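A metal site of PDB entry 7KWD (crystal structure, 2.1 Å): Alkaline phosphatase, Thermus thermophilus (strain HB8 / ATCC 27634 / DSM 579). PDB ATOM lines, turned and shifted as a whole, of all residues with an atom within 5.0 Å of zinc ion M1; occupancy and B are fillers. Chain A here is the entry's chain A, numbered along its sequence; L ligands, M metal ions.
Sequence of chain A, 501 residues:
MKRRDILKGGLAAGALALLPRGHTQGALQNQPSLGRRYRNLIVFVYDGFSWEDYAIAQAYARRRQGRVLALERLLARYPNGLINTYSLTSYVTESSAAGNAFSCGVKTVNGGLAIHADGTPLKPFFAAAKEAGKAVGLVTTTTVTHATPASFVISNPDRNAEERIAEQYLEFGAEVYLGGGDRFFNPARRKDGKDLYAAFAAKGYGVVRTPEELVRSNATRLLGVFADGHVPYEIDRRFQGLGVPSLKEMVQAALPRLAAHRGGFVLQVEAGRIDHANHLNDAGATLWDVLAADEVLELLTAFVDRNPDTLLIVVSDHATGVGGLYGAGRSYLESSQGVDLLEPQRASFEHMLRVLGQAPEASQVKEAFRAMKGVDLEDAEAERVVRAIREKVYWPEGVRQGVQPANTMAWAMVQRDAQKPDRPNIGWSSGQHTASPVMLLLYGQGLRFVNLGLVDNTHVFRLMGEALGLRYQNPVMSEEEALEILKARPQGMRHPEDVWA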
ATOM      1  N   ASP A  47       3.531  19.835   5.301  1.00  0.00           N
ATOM      2  CA  ASP A  47       2.281  19.928   4.569  1.00  0.00           C
ATOM      3  C   ASP A  47       1.442  18.678   4.779  1.00  0.00           C
ATOM      4  O   ASP A  47       1.907  17.566   4.566  1.00  0.00           O
ATOM      5  CB  ASP A  47       2.558  20.141   3.078  1.00  0.00           C
ATOM      6  CG  ASP A  47       1.388  20.734   2.387  1.00  0.00           C
ATOM      7  OD1 ASP A  47       0.315  20.109   2.491  1.00  0.00           O
ATOM      8  OD2 ASP A  47       1.524  21.827   1.771  1.00  0.00           O
ATOM      9  N   ASP A 275       1.609  15.531   2.740  1.00  0.00           N
ATOM     10  CA  ASP A 275       0.254  15.690   2.206  1.00  0.00           C
ATOM     11  C   ASP A 275      -0.028  14.688   1.104  1.00  0.00           C
ATOM     12  O   ASP A 275      -1.014  13.945   1.156  1.00  0.00           O
ATOM     13  CB  ASP A 275       0.094  17.134   1.701  1.00  0.00           C
ATOM     14  CG  ASP A 275      -1.274  17.442   1.188  1.00  0.00           C
ATOM     15  OD1 ASP A 275      -2.237  17.325   1.993  1.00  0.00           O
ATOM     16  OD2 ASP A 275      -1.382  17.816  -0.006  1.00  0.00           O
ATOM     17  N   HIS A 279      -2.741  11.725   0.860  1.00  0.00           N
ATOM     18  CA  HIS A 279      -3.737  11.629  -0.214  1.00  0.00           C
ATOM     19  C   HIS A 279      -3.775  10.210  -0.798  1.00  0.00           C
ATOM     20  O   HIS A 279      -4.863   9.655  -1.006  1.00  0.00           O
ATOM     21  CB  HIS A 279      -3.400  12.631  -1.323  1.00  0.00           C
ATOM     22  CG  HIS A 279      -3.877  14.024  -1.047  1.00  0.00           C
ATOM     23  ND1 HIS A 279      -5.191  14.305  -0.731  1.00  0.00           N
ATOM     24  CD2 HIS A 279      -3.225  15.208  -1.042  1.00  0.00           C
ATOM     25  CE1 HIS A 279      -5.321  15.611  -0.564  1.00  0.00           C
ATOM     26  NE2 HIS A 279      -4.152  16.178  -0.768  1.00  0.00           N
ATOM     27  N   HIS A 318      -2.257  21.937   7.493  1.00  0.00           N
ATOM     28  CA  HIS A 318      -3.540  21.297   7.739  1.00  0.00           C
ATOM     29  C   HIS A 318      -3.260  19.790   7.825  1.00  0.00           C
ATOM     30  O   HIS A 318      -2.207  19.306   7.382  1.00  0.00           O
ATOM     31  CB  HIS A 318      -4.567  21.535   6.622  1.00  0.00           C
ATOM     32  CG  HIS A 318      -4.012  21.173   5.291  1.00  0.00           C
ATOM     33  ND1 HIS A 318      -3.932  19.872   4.848  1.00  0.00           N
ATOM     34  CD2 HIS A 318      -3.398  21.926   4.363  1.00  0.00           C
ATOM     35  CE1 HIS A 318      -3.331  19.847   3.680  1.00  0.00           C
ATOM     36  NE2 HIS A 318      -3.013  21.081   3.358  1.00  0.00           N
ATOM     37  N   THR A 320      -4.283  15.861   6.686  1.00  0.00           N
ATOM     38  CA  THR A 320      -4.747  15.170   5.492  1.00  0.00           C
ATOM     39  C   THR A 320      -4.885  13.680   5.757  1.00  0.00           C
ATOM     40  O   THR A 320      -3.978  13.057   6.326  1.00  0.00           O
ATOM     41  CB  THR A 320      -3.815  15.416   4.309  1.00  0.00           C
ATOM     42  OG1 THR A 320      -3.805  16.807   4.054  1.00  0.00           O
ATOM     43  CG2 THR A 320      -4.291  14.662   3.040  1.00  0.00           C
ATOM     44  N   HIS A 433      -7.946  16.472   2.590  1.00  0.00           N
ATOM     45  CA  HIS A 433      -7.657  17.224   3.811  1.00  0.00           C
ATOM     46  C   HIS A 433      -8.789  17.090   4.818  1.00  0.00           C
ATOM     47  O   HIS A 433      -9.943  16.825   4.459  1.00  0.00           O
ATOM     48  CB  HIS A 433      -7.471  18.713   3.537  1.00  0.00           C
ATOM     49  CG  HIS A 433      -6.464  19.002   2.498  1.00  0.00           C
ATOM     50  ND1 HIS A 433      -6.236  20.268   2.010  1.00  0.00           N
ATOM     51  CD2 HIS A 433      -5.605  18.181   1.822  1.00  0.00           C
ATOM     52  CE1 HIS A 433      -5.292  20.225   1.083  1.00  0.00           C
ATOM     53  NE2 HIS A 433      -4.910  18.977   0.944  1.00  0.00           N
HETATM   54  O1  LIG L   1      -2.231  18.103  -3.518  1.00  0.00           O
HETATM   55  O2  LIG L   1      -3.025  19.723  -4.765  1.00  0.00           O
HETATM   56  C1  LIG L   1      -3.007  19.092  -3.665  1.00  0.00           C
HETATM   57  C2  LIG L   1      -3.919  19.530  -2.486  1.00  0.00           C
HETATM   58  O3  LIG L   1      -5.267  19.685  -2.877  1.00  0.00           O
HETATM   59  C3  LIG L   1      -3.363  20.895  -2.094  1.00  0.00           C
HETATM   60  O4  LIG L   1      -4.276  21.720  -1.421  1.00  0.00           O
HETATM   61  C4  LIG L   1      -2.167  20.860  -1.178  1.00  0.00           C
HETATM   62  O5  LIG L   1      -1.099  21.369  -1.591  1.00  0.00           O
HETATM   63  O6  LIG L   1      -2.252  20.333  -0.037  1.00  0.00           O
HETATM   64 ZN    ZN M   1      -3.308  18.180  -0.312  1.00  0.00          ZN
HETATM   65 ZN    ZN M   2      -1.178  21.716   2.240  1.00  0.00          ZN
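OG1 of Thr 320 is in hydrogen-bond range of OD1 of Asp 275 (2.6 Å). N of Asp 275 is in hydrogen-bond range of O of Asp 47 (2.8 Å).
Of the 6 residues printed, 3 come within 4 Å of zinc ion M1.
Zinc ion M1 is bound by the side-chain carboxylate (OD2) of Asp 275 (2.0 Å). NE2 of His 433 binds zinc ion M1, 2.2 Å away. Zinc ion M1 is bound by a ring nitrogen (NE2) of His 279. Zinc ion M1 is bound by O6 of the ligand, at 2.4 Å. Zinc ion M1 has four donor atoms within binding distance. Slightly farther from zinc ion M1 lies the side-chain carboxylate (OD1) of Asp 275 (2.7 Å).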
